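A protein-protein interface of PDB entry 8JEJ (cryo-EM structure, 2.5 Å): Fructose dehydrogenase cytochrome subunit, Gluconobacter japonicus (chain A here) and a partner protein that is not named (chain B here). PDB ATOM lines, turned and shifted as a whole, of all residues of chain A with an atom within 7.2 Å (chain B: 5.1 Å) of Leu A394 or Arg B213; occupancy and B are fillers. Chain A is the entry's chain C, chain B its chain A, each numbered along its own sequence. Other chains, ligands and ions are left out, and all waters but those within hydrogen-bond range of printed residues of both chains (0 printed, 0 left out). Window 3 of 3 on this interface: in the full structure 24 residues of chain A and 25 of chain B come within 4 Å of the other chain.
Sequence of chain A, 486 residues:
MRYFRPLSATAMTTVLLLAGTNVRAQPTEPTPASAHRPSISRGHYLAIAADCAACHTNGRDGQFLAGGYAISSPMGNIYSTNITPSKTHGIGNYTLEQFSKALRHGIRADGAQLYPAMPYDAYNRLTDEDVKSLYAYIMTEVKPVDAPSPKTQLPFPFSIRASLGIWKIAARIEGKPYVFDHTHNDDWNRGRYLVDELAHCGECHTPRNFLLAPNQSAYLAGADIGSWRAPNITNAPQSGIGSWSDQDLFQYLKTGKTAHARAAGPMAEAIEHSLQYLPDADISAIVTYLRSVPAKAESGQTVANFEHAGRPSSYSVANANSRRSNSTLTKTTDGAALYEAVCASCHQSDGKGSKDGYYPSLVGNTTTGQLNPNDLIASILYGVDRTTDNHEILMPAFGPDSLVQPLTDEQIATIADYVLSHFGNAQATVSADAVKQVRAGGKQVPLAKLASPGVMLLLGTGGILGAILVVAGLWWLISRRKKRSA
Pro B209 touches Glu A392.
Pro B209 touches Leu A394 (CB to CB, 3.7 Å).
Gly B212 touches Leu A394 (O to CD2, 3.6 Å).
Arg B213 touches Leu A394.
N of Pro B214 touches CD2 of Leu A394 (3.7 Å).
Pro A396 touches Pro B214.
Asp B211 touches Leu A403 (OD2 to CD1, 3.6 Å).
Tyr B236 touches Leu A403.
Gly B229 touches Val A404 (CA to CG2, 3.99 Å).
Of chain B, only Pro B209 (3.7 Å), Gly B212 (3.6 Å), Arg B213 (3.5 Å) and Pro B214 (3.7 Å) come within 4 Å of Leu A394.
Printed residues of chain A within 4 Å of Arg B213: Leu A394 (3.5 Å).
Printed residues of chain A within 4 Å of Gly B212: Leu A394 (3.6 Å).
Printed residues of chain B within 4 Å of Val A404: Gly B229.
Printed residues of chain B within 4 Å of Leu A403: Asp B211 and Tyr B236.
Of the printed residues of chain A, Gly B229 touches Val A404 (3.99 Å).
Printed residues of chain A within 4 Å of Pro B209: Glu A392 and Leu A394.
Of the printed residues of chain A, Pro B214 touches Leu A394 and Pro A396.
Met B153 touches none of the printed residues of chain A.
Met B231 touches none of the printed residues of chain A.
Printed residues of chain B that touch a printed residue of chain A: Pro B209, Asp B211, Gly B212, Arg B213, Pro B214, Gly B229 and Tyr B236.
Hydrophobic or aromatic side chains of chain B that line the printed part of chain A: Pro B209, Pro B214 and Tyr B236.
Among the printed residues, 9 pairs touch across the chains.
NE of Arg B213 is in salt-bridge range of OD2 of Asp B211.
ND2 of Asn B206 sits at hydrogen-bond distance from O of Arg B213 (3.4 Å).
The side-chain carboxylate of Glu A392 sits close to the side-chain carboxylate of Asp A385, 2.7 Å away.
The guanidinium group (NH1) of Arg B213 is in hydrogen-bond range of the backbone carbonyl oxygen (O) of Met B231, 3.3 Å away.
ND2 of Asn B206 sits at hydrogen-bond distance from O of Pro B214 (3.0 Å).
The side-chain hydroxyl of Tyr B236 sits at hydrogen-bond distance from the backbone carbonyl oxygen of Met B231 (3.0 Å).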
ATOM      1  N   CYS A 346      27.538   4.676  17.264  1.00  0.00           N
ATOM      2  CA  CYS A 346      28.328   3.879  16.331  1.00  0.00           C
ATOM      3  C   CYS A 346      29.826   4.061  16.560  1.00  0.00           C
ATOM      4  O   CYS A 346      30.531   3.102  16.885  1.00  0.00           O
ATOM      5  CB  CYS A 346      27.952   4.243  14.894  1.00  0.00           C
ATOM      6  SG  CYS A 346      26.212   3.982  14.494  1.00  0.00           S
ATOM      7  N   TYR A 358      33.708  -2.012  11.483  1.00  0.00           N
ATOM      8  CA  TYR A 358      32.581  -1.567  10.671  1.00  0.00           C
ATOM      9  C   TYR A 358      32.329  -0.080  10.872  1.00  0.00           C
ATOM     10  O   TYR A 358      32.119   0.665   9.908  1.00  0.00           O
ATOM     11  CB  TYR A 358      31.326  -2.372  11.004  1.00  0.00           C
ATOM     12  CG  TYR A 358      30.187  -2.098  10.050  1.00  0.00           C
ATOM     13  CD1 TYR A 358      29.319  -1.033  10.256  1.00  0.00           C
ATOM     14  CD2 TYR A 358      29.994  -2.890   8.929  1.00  0.00           C
ATOM     15  CE1 TYR A 358      28.289  -0.773   9.379  1.00  0.00           C
ATOM     16  CE2 TYR A 358      28.964  -2.639   8.050  1.00  0.00           C
ATOM     17  CZ  TYR A 358      28.115  -1.580   8.278  1.00  0.00           C
ATOM     18  OH  TYR A 358      27.087  -1.329   7.401  1.00  0.00           O
ATOM     19  N   TYR A 359      32.341   0.369  12.121  1.00  0.00           N
ATOM     20  CA  TYR A 359      32.237   1.786  12.413  1.00  0.00           C
ATOM     21  C   TYR A 359      33.642   2.333  12.588  1.00  0.00           C
ATOM     22  O   TYR A 359      34.334   1.940  13.538  1.00  0.00           O
ATOM     23  CB  TYR A 359      31.397   2.020  13.663  1.00  0.00           C
ATOM     24  CG  TYR A 359      29.977   1.542  13.483  1.00  0.00           C
ATOM     25  CD1 TYR A 359      29.200   2.023  12.441  1.00  0.00           C
ATOM     26  CD2 TYR A 359      29.425   0.592  14.330  1.00  0.00           C
ATOM     27  CE1 TYR A 359      27.911   1.589  12.256  1.00  0.00           C
ATOM     28  CE2 TYR A 359      28.130   0.151  14.151  1.00  0.00           C
ATOM     29  CZ  TYR A 359      27.379   0.656  13.111  1.00  0.00           C
ATOM     30  OH  TYR A 359      26.089   0.233  12.912  1.00  0.00           O
ATOM     31  N   TYR A 382      26.173  14.616   4.641  1.00  0.00           N
ATOM     32  CA  TYR A 382      25.650  13.678   3.661  1.00  0.00           C
ATOM     33  C   TYR A 382      25.798  12.219   4.062  1.00  0.00           C
ATOM     34  O   TYR A 382      25.206  11.357   3.405  1.00  0.00           O
ATOM     35  CB  TYR A 382      26.336  13.900   2.306  1.00  0.00           C
ATOM     36  CG  TYR A 382      26.260  15.326   1.822  1.00  0.00           C
ATOM     37  CD1 TYR A 382      25.038  15.916   1.531  1.00  0.00           C
ATOM     38  CD2 TYR A 382      27.408  16.090   1.668  1.00  0.00           C
ATOM     39  CE1 TYR A 382      24.962  17.218   1.094  1.00  0.00           C
ATOM     40  CE2 TYR A 382      27.341  17.397   1.233  1.00  0.00           C
ATOM     41  CZ  TYR A 382      26.116  17.956   0.946  1.00  0.00           C
ATOM     42  OH  TYR A 382      26.041  19.257   0.510  1.00  0.00           O
ATOM     43  N   GLY A 383      26.553  11.919   5.109  1.00  0.00           N
ATOM     44  CA  GLY A 383      26.791  10.538   5.461  1.00  0.00           C
ATOM     45  C   GLY A 383      27.755   9.875   4.493  1.00  0.00           C
ATOM     46  O   GLY A 383      28.501  10.526   3.756  1.00  0.00           O
ATOM     47  N   VAL A 384      27.739   8.547   4.514  1.00  0.00           N
ATOM     48  CA  VAL A 384      28.569   7.731   3.636  1.00  0.00           C
ATOM     49  C   VAL A 384      27.688   6.656   3.021  1.00  0.00           C
ATOM     50  O   VAL A 384      26.790   6.132   3.683  1.00  0.00           O
ATOM     51  CB  VAL A 384      29.757   7.094   4.393  1.00  0.00           C
ATOM     52  CG1 VAL A 384      30.685   6.373   3.430  1.00  0.00           C
ATOM     53  CG2 VAL A 384      30.523   8.144   5.181  1.00  0.00           C
ATOM     54  N   ASP A 385      27.934   6.333   1.757  1.00  0.00           N
ATOM     55  CA  ASP A 385      27.197   5.257   1.099  1.00  0.00           C
ATOM     56  C   ASP A 385      28.121   4.631   0.066  1.00  0.00           C
ATOM     57  O   ASP A 385      28.431   5.263  -0.946  1.00  0.00           O
ATOM     58  CB  ASP A 385      25.920   5.784   0.454  1.00  0.00           C
ATOM     59  CG  ASP A 385      24.952   4.680   0.094  1.00  0.00           C
ATOM     60  OD1 ASP A 385      25.319   3.497   0.240  1.00  0.00           O
ATOM     61  OD2 ASP A 385      23.825   4.994  -0.338  1.00  0.00           O
ATOM     62  N   ARG A 386      28.558   3.397   0.315  1.00  0.00           N
ATOM     63  CA  ARG A 386      29.535   2.754  -0.562  1.00  0.00           C
ATOM     64  C   ARG A 386      29.232   1.270  -0.681  1.00  0.00           C
ATOM     65  O   ARG A 386      29.292   0.546   0.313  1.00  0.00           O
ATOM     66  CB  ARG A 386      30.962   2.963  -0.047  1.00  0.00           C
ATOM     67  CG  ARG A 386      32.047   2.592  -1.050  1.00  0.00           C
ATOM     68  CD  ARG A 386      33.351   2.239  -0.351  1.00  0.00           C
ATOM     69  NE  ARG A 386      33.459   2.881   0.953  1.00  0.00           N
ATOM     70  CZ  ARG A 386      33.673   2.238   2.092  1.00  0.00           C
ATOM     71  NH1 ARG A 386      33.819   0.925   2.128  1.00  0.00           N
ATOM     72  NH2 ARG A 386      33.740   2.931   3.225  1.00  0.00           N
ATOM     73  N   GLU A 392      26.880  -3.070   1.250  1.00  0.00           N
ATOM     74  CA  GLU A 392      26.676  -1.627   1.308  1.00  0.00           C
ATOM     75  C   GLU A 392      27.028  -1.078   2.687  1.00  0.00           C
ATOM     76  O   GLU A 392      26.394  -1.429   3.687  1.00  0.00           O
ATOM     77  CB  GLU A 392      25.239  -1.269   0.942  1.00  0.00           C
ATOM     78  CG  GLU A 392      25.079   0.167   0.479  1.00  0.00           C
ATOM     79  CD  GLU A 392      23.638   0.618   0.463  1.00  0.00           C
ATOM     80  OE1 GLU A 392      22.784  -0.127  -0.058  1.00  0.00           O
ATOM     81  OE2 GLU A 392      23.358   1.723   0.967  1.00  0.00           O
ATOM     82  N   ILE A 393      28.057  -0.229   2.725  1.00  0.00           N
ATOM     83  CA  ILE A 393      28.275   0.713   3.813  1.00  0.00           C
ATOM     84  C   ILE A 393      27.255   1.836   3.733  1.00  0.00           C
ATOM     85  O   ILE A 393      26.982   2.369   2.645  1.00  0.00           O
ATOM     86  CB  ILE A 393      29.695   1.304   3.728  1.00  0.00           C
ATOM     87  CG1 ILE A 393      30.701   0.564   4.625  1.00  0.00           C
ATOM     88  CG2 ILE A 393      29.651   2.812   3.852  1.00  0.00           C
ATOM     89  CD1 ILE A 393      30.699  -0.952   4.403  1.00  0.00           C
ATOM     90  N   LEU A 394      26.728   2.240   4.889  1.00  0.00           N
ATOM     91  CA  LEU A 394      25.947   3.468   4.963  1.00  0.00           C
ATOM     92  C   LEU A 394      26.064   4.083   6.351  1.00  0.00           C
ATOM     93  O   LEU A 394      25.764   3.431   7.353  1.00  0.00           O
ATOM     94  CB  LEU A 394      24.480   3.214   4.619  1.00  0.00           C
ATOM     95  CG  LEU A 394      23.668   4.475   4.311  1.00  0.00           C
ATOM     96  CD1 LEU A 394      22.770   4.256   3.108  1.00  0.00           C
ATOM     97  CD2 LEU A 394      22.856   4.905   5.518  1.00  0.00           C
ATOM     98  N   MET A 395      26.507   5.323   6.392  1.00  0.00           N
ATOM     99  CA  MET A 395      26.313   6.293   7.460  1.00  0.00           C
ATOM    100  C   MET A 395      25.199   7.243   7.066  1.00  0.00           C
ATOM    101  O   MET A 395      25.284   7.869   5.997  1.00  0.00           O
ATOM    102  CB  MET A 395      27.574   7.100   7.709  1.00  0.00           C
ATOM    103  CG  MET A 395      27.315   8.305   8.589  1.00  0.00           C
ATOM    104  SD  MET A 395      28.821   9.235   8.809  1.00  0.00           S
ATOM    105  CE  MET A 395      28.205  10.792   9.417  1.00  0.00           C
ATOM    106  N   PRO A 396      24.172   7.405   7.894  1.00  0.00           N
ATOM    107  CA  PRO A 396      23.062   8.290   7.528  1.00  0.00           C
ATOM    108  C   PRO A 396      23.490   9.748   7.451  1.00  0.00           C
ATOM    109  O   PRO A 396      24.446  10.181   8.097  1.00  0.00           O
ATOM    110  CB  PRO A 396      22.048   8.070   8.655  1.00  0.00           C
ATOM    111  CG  PRO A 396      22.867   7.608   9.809  1.00  0.00           C
ATOM    112  CD  PRO A 396      23.990   6.807   9.227  1.00  0.00           C
ATOM    113  N   ALA A 397      22.766  10.504   6.630  1.00  0.00           N
ATOM    114  CA  ALA A 397      22.982  11.938   6.543  1.00  0.00           C
ATOM    115  C   ALA A 397      22.455  12.634   7.792  1.00  0.00           C
ATOM    116  O   ALA A 397      21.516  12.165   8.443  1.00  0.00           O
ATOM    117  CB  ALA A 397      22.303  12.509   5.300  1.00  0.00           C
ATOM    118  N   LEU A 403      16.729  12.132   7.735  1.00  0.00           N
ATOM    119  CA  LEU A 403      15.606  11.405   8.311  1.00  0.00           C
ATOM    120  C   LEU A 403      15.856  10.996   9.753  1.00  0.00           C
ATOM    121  O   LEU A 403      14.906  10.892  10.535  1.00  0.00           O
ATOM    122  CB  LEU A 403      15.305  10.150   7.488  1.00  0.00           C
ATOM    123  CG  LEU A 403      14.413  10.263   6.254  1.00  0.00           C
ATOM    124  CD1 LEU A 403      13.965   8.881   5.823  1.00  0.00           C
ATOM    125  CD2 LEU A 403      13.216  11.153   6.526  1.00  0.00           C
ATOM    126  N   VAL A 404      17.114  10.763  10.120  1.00  0.00           N
ATOM    127  CA  VAL A 404      17.433  10.266  11.455  1.00  0.00           C
ATOM    128  C   VAL A 404      17.489  11.411  12.457  1.00  0.00           C
ATOM    129  O   VAL A 404      16.773  11.413  13.464  1.00  0.00           O
ATOM    130  CB  VAL A 404      18.752   9.473  11.428  1.00  0.00           C
ATOM    131  CG1 VAL A 404      19.171   9.084  12.834  1.00  0.00           C
ATOM    132  CG2 VAL A 404      18.608   8.243  10.546  1.00  0.00           C
ATOM    133  N   MET B 153       7.897   1.336   4.580  1.00  0.00           N
ATOM    134  CA  MET B 153       8.458   1.249   5.920  1.00  0.00           C
ATOM    135  C   MET B 153       9.726   0.411   5.997  1.00  0.00           C
ATOM    136  O   MET B 153      10.422   0.469   7.016  1.00  0.00           O
ATOM    137  CB  MET B 153       7.418   0.679   6.888  1.00  0.00           C
ATOM    138  CG  MET B 153       6.184   1.548   7.053  1.00  0.00           C
ATOM    139  SD  MET B 153       4.767   0.617   7.657  1.00  0.00           S
ATOM    140  CE  MET B 153       5.399   0.032   9.224  1.00  0.00           C
ATOM    141  N   GLY B 154      10.046  -0.359   4.961  1.00  0.00           N
ATOM    142  CA  GLY B 154      11.239  -1.182   4.992  1.00  0.00           C
ATOM    143  C   GLY B 154      11.144  -2.332   5.969  1.00  0.00           C
ATOM    144  O   GLY B 154      11.831  -2.342   6.993  1.00  0.00           O
ATOM    145  N   ASN B 206      16.140  -2.591   9.448  1.00  0.00           N
ATOM    146  CA  ASN B 206      17.062  -2.674   8.317  1.00  0.00           C
ATOM    147  C   ASN B 206      18.051  -3.811   8.547  1.00  0.00           C
ATOM    148  O   ASN B 206      18.992  -3.681   9.332  1.00  0.00           O
ATOM    149  CB  ASN B 206      17.786  -1.346   8.123  1.00  0.00           C
ATOM    150  CG  ASN B 206      16.912  -0.297   7.472  1.00  0.00           C
ATOM    151  OD1 ASN B 206      15.828  -0.596   6.977  1.00  0.00           O
ATOM    152  ND2 ASN B 206      17.379   0.944   7.471  1.00  0.00           N
ATOM    153  N   ARG B 208      19.771  -4.542   6.033  1.00  0.00           N
ATOM    154  CA  ARG B 208      20.768  -3.950   5.158  1.00  0.00           C
ATOM    155  C   ARG B 208      20.438  -2.472   5.054  1.00  0.00           C
ATOM    156  O   ARG B 208      19.334  -2.060   5.426  1.00  0.00           O
ATOM    157  CB  ARG B 208      20.766  -4.611   3.773  1.00  0.00           C
ATOM    158  CG  ARG B 208      19.445  -4.501   3.040  1.00  0.00           C
ATOM    159  CD  ARG B 208      19.507  -5.202   1.701  1.00  0.00           C
ATOM    160  NE  ARG B 208      18.202  -5.258   1.056  1.00  0.00           N
ATOM    161  CZ  ARG B 208      17.660  -4.258   0.376  1.00  0.00           C
ATOM    162  NH1 ARG B 208      18.282  -3.098   0.241  1.00  0.00           N
ATOM    163  NH2 ARG B 208      16.465  -4.424  -0.182  1.00  0.00           N
ATOM    164  N   PRO B 209      21.375  -1.644   4.597  1.00  0.00           N
ATOM    165  CA  PRO B 209      21.048  -0.228   4.398  1.00  0.00           C
ATOM    166  C   PRO B 209      19.834  -0.074   3.495  1.00  0.00           C
ATOM    167  O   PRO B 209      19.726  -0.718   2.450  1.00  0.00           O
ATOM    168  CB  PRO B 209      22.317   0.339   3.757  1.00  0.00           C
ATOM    169  CG  PRO B 209      23.396  -0.527   4.267  1.00  0.00           C
ATOM    170  CD  PRO B 209      22.810  -1.906   4.386  1.00  0.00           C
ATOM    171  N   TYR B 210      18.908   0.783   3.913  1.00  0.00           N
ATOM    172  CA  TYR B 210      17.603   0.862   3.278  1.00  0.00           C
ATOM    173  C   TYR B 210      17.006   2.232   3.553  1.00  0.00           C
ATOM    174  O   TYR B 210      17.066   2.719   4.685  1.00  0.00           O
ATOM    175  CB  TYR B 210      16.681  -0.246   3.802  1.00  0.00           C
ATOM    176  CG  TYR B 210      15.403  -0.433   3.022  1.00  0.00           C
ATOM    177  CD1 TYR B 210      14.303   0.380   3.252  1.00  0.00           C
ATOM    178  CD2 TYR B 210      15.289  -1.433   2.068  1.00  0.00           C
ATOM    179  CE1 TYR B 210      13.136   0.214   2.546  1.00  0.00           C
ATOM    180  CE2 TYR B 210      14.121  -1.611   1.360  1.00  0.00           C
ATOM    181  CZ  TYR B 210      13.046  -0.786   1.605  1.00  0.00           C
ATOM    182  OH  TYR B 210      11.876  -0.953   0.904  1.00  0.00           O
ATOM    183  N   ASP B 211      16.430   2.842   2.515  1.00  0.00           N
ATOM    184  CA  ASP B 211      15.800   4.158   2.617  1.00  0.00           C
ATOM    185  C   ASP B 211      16.789   5.223   3.081  1.00  0.00           C
ATOM    186  O   ASP B 211      16.423   6.168   3.782  1.00  0.00           O
ATOM    187  CB  ASP B 211      14.580   4.112   3.544  1.00  0.00           C
ATOM    188  CG  ASP B 211      13.669   5.310   3.377  1.00  0.00           C
ATOM    189  OD1 ASP B 211      13.625   5.879   2.267  1.00  0.00           O
ATOM    190  OD2 ASP B 211      12.999   5.684   4.362  1.00  0.00           O
ATOM    191  N   GLY B 212      18.055   5.079   2.695  1.00  0.00           N
ATOM    192  CA  GLY B 212      19.068   6.012   3.144  1.00  0.00           C
ATOM    193  C   GLY B 212      19.345   5.965   4.626  1.00  0.00           C
ATOM    194  O   GLY B 212      19.907   6.915   5.173  1.00  0.00           O
ATOM    195  N   ARG B 213      18.971   4.876   5.294  1.00  0.00           N
ATOM    196  CA  ARG B 213      19.126   4.722   6.727  1.00  0.00           C
ATOM    197  C   ARG B 213      20.009   3.518   7.028  1.00  0.00           C
ATOM    198  O   ARG B 213      20.080   2.581   6.227  1.00  0.00           O
ATOM    199  CB  ARG B 213      17.760   4.561   7.406  1.00  0.00           C
ATOM    200  CG  ARG B 213      16.864   5.773   7.239  1.00  0.00           C
ATOM    201  CD  ARG B 213      15.579   5.636   8.023  1.00  0.00           C
ATOM    202  NE  ARG B 213      14.601   4.804   7.334  1.00  0.00           N
ATOM    203  CZ  ARG B 213      14.242   3.591   7.728  1.00  0.00           C
ATOM    204  NH1 ARG B 213      14.768   3.032   8.804  1.00  0.00           N
ATOM    205  NH2 ARG B 213      13.332   2.923   7.025  1.00  0.00           N
ATOM    206  N   PRO B 214      20.702   3.516   8.166  1.00  0.00           N
ATOM    207  CA  PRO B 214      21.720   2.488   8.407  1.00  0.00           C
ATOM    208  C   PRO B 214      21.119   1.120   8.685  1.00  0.00           C
ATOM    209  O   PRO B 214      19.951   0.972   9.048  1.00  0.00           O
ATOM    210  CB  PRO B 214      22.467   3.018   9.634  1.00  0.00           C
ATOM    211  CG  PRO B 214      21.458   3.836  10.342  1.00  0.00           C
ATOM    212  CD  PRO B 214      20.651   4.497   9.264  1.00  0.00           C
ATOM    213  N   GLN B 215      21.957   0.105   8.497  1.00  0.00           N
ATOM    214  CA  GLN B 215      21.617  -1.254   8.883  1.00  0.00           C
ATOM    215  C   GLN B 215      21.612  -1.388  10.403  1.00  0.00           C
ATOM    216  O   GLN B 215      22.403  -0.756  11.108  1.00  0.00           O
ATOM    217  CB  GLN B 215      22.614  -2.237   8.270  1.00  0.00           C
ATOM    218  CG  GLN B 215      22.397  -3.690   8.637  1.00  0.00           C
ATOM    219  CD  GLN B 215      23.348  -4.612   7.907  1.00  0.00           C
ATOM    220  OE1 GLN B 215      23.876  -4.264   6.853  1.00  0.00           O
ATOM    221  NE2 GLN B 215      23.578  -5.791   8.468  1.00  0.00           N
ATOM    222  N   GLY B 229      18.284   5.279  13.845  1.00  0.00           N
ATOM    223  CA  GLY B 229      17.303   5.205  12.777  1.00  0.00           C
ATOM    224  C   GLY B 229      17.437   3.996  11.878  1.00  0.00           C
ATOM    225  O   GLY B 229      17.261   4.111  10.659  1.00  0.00           O
ATOM    226  N   ALA B 230      17.739   2.835  12.448  1.00  0.00           N
ATOM    227  CA  ALA B 230      17.794   1.591  11.694  1.00  0.00           C
ATOM    228  C   ALA B 230      16.445   0.890  11.633  1.00  0.00           C
ATOM    229  O   ALA B 230      16.354  -0.212  11.084  1.00  0.00           O
ATOM    230  CB  ALA B 230      18.840   0.656  12.297  1.00  0.00           C
ATOM    231  N   MET B 231      15.406   1.502  12.192  1.00  0.00           N
ATOM    232  CA  MET B 231      14.052   0.983  12.172  1.00  0.00           C
ATOM    233  C   MET B 231      13.108   2.109  11.778  1.00  0.00           C
ATOM    234  O   MET B 231      13.472   3.287  11.793  1.00  0.00           O
ATOM    235  CB  MET B 231      13.663   0.399  13.532  1.00  0.00           C
ATOM    236  CG  MET B 231      13.751   1.402  14.662  1.00  0.00           C
ATOM    237  SD  MET B 231      13.290   0.700  16.247  1.00  0.00           S
ATOM    238  CE  MET B 231      11.569   1.175  16.304  1.00  0.00           C
ATOM    239  N   TYR B 232      11.882   1.744  11.421  1.00  0.00           N
ATOM    240  CA  TYR B 232      10.932   2.731  10.933  1.00  0.00           C
ATOM    241  C   TYR B 232      10.281   3.502  12.071  1.00  0.00           C
ATOM    242  O   TYR B 232       9.871   2.926  13.083  1.00  0.00           O
ATOM    243  CB  TYR B 232       9.846   2.076  10.084  1.00  0.00           C
ATOM    244  CG  TYR B 232       9.013   3.102   9.361  1.00  0.00           C
ATOM    245  CD1 TYR B 232       9.510   3.754   8.244  1.00  0.00           C
ATOM    246  CD2 TYR B 232       7.748   3.450   9.816  1.00  0.00           C
ATOM    247  CE1 TYR B 232       8.768   4.703   7.586  1.00  0.00           C
ATOM    248  CE2 TYR B 232       6.997   4.402   9.163  1.00  0.00           C
ATOM    249  CZ  TYR B 232       7.514   5.025   8.049  1.00  0.00           C
ATOM    250  OH  TYR B 232       6.777   5.973   7.388  1.00  0.00           O
ATOM    251  N   TYR B 236       9.485   9.660   9.779  1.00  0.00           N
ATOM    252  CA  TYR B 236      10.027   9.596   8.423  1.00  0.00           C
ATOM    253  C   TYR B 236       8.976  10.000   7.400  1.00  0.00           C
ATOM    254  O   TYR B 236       9.239  10.813   6.505  1.00  0.00           O
ATOM    255  CB  TYR B 236      10.537   8.189   8.111  1.00  0.00           C
ATOM    256  CG  TYR B 236      11.591   7.659   9.047  1.00  0.00           C
ATOM    257  CD1 TYR B 236      12.411   8.516   9.768  1.00  0.00           C
ATOM    258  CD2 TYR B 236      11.769   6.294   9.206  1.00  0.00           C
ATOM    259  CE1 TYR B 236      13.372   8.024  10.622  1.00  0.00           C
ATOM    260  CE2 TYR B 236      12.724   5.796  10.054  1.00  0.00           C
ATOM    261  CZ  TYR B 236      13.524   6.662  10.759  1.00  0.00           C
ATOM    262  OH  TYR B 236      14.477   6.156  11.605  1.00  0.00           O
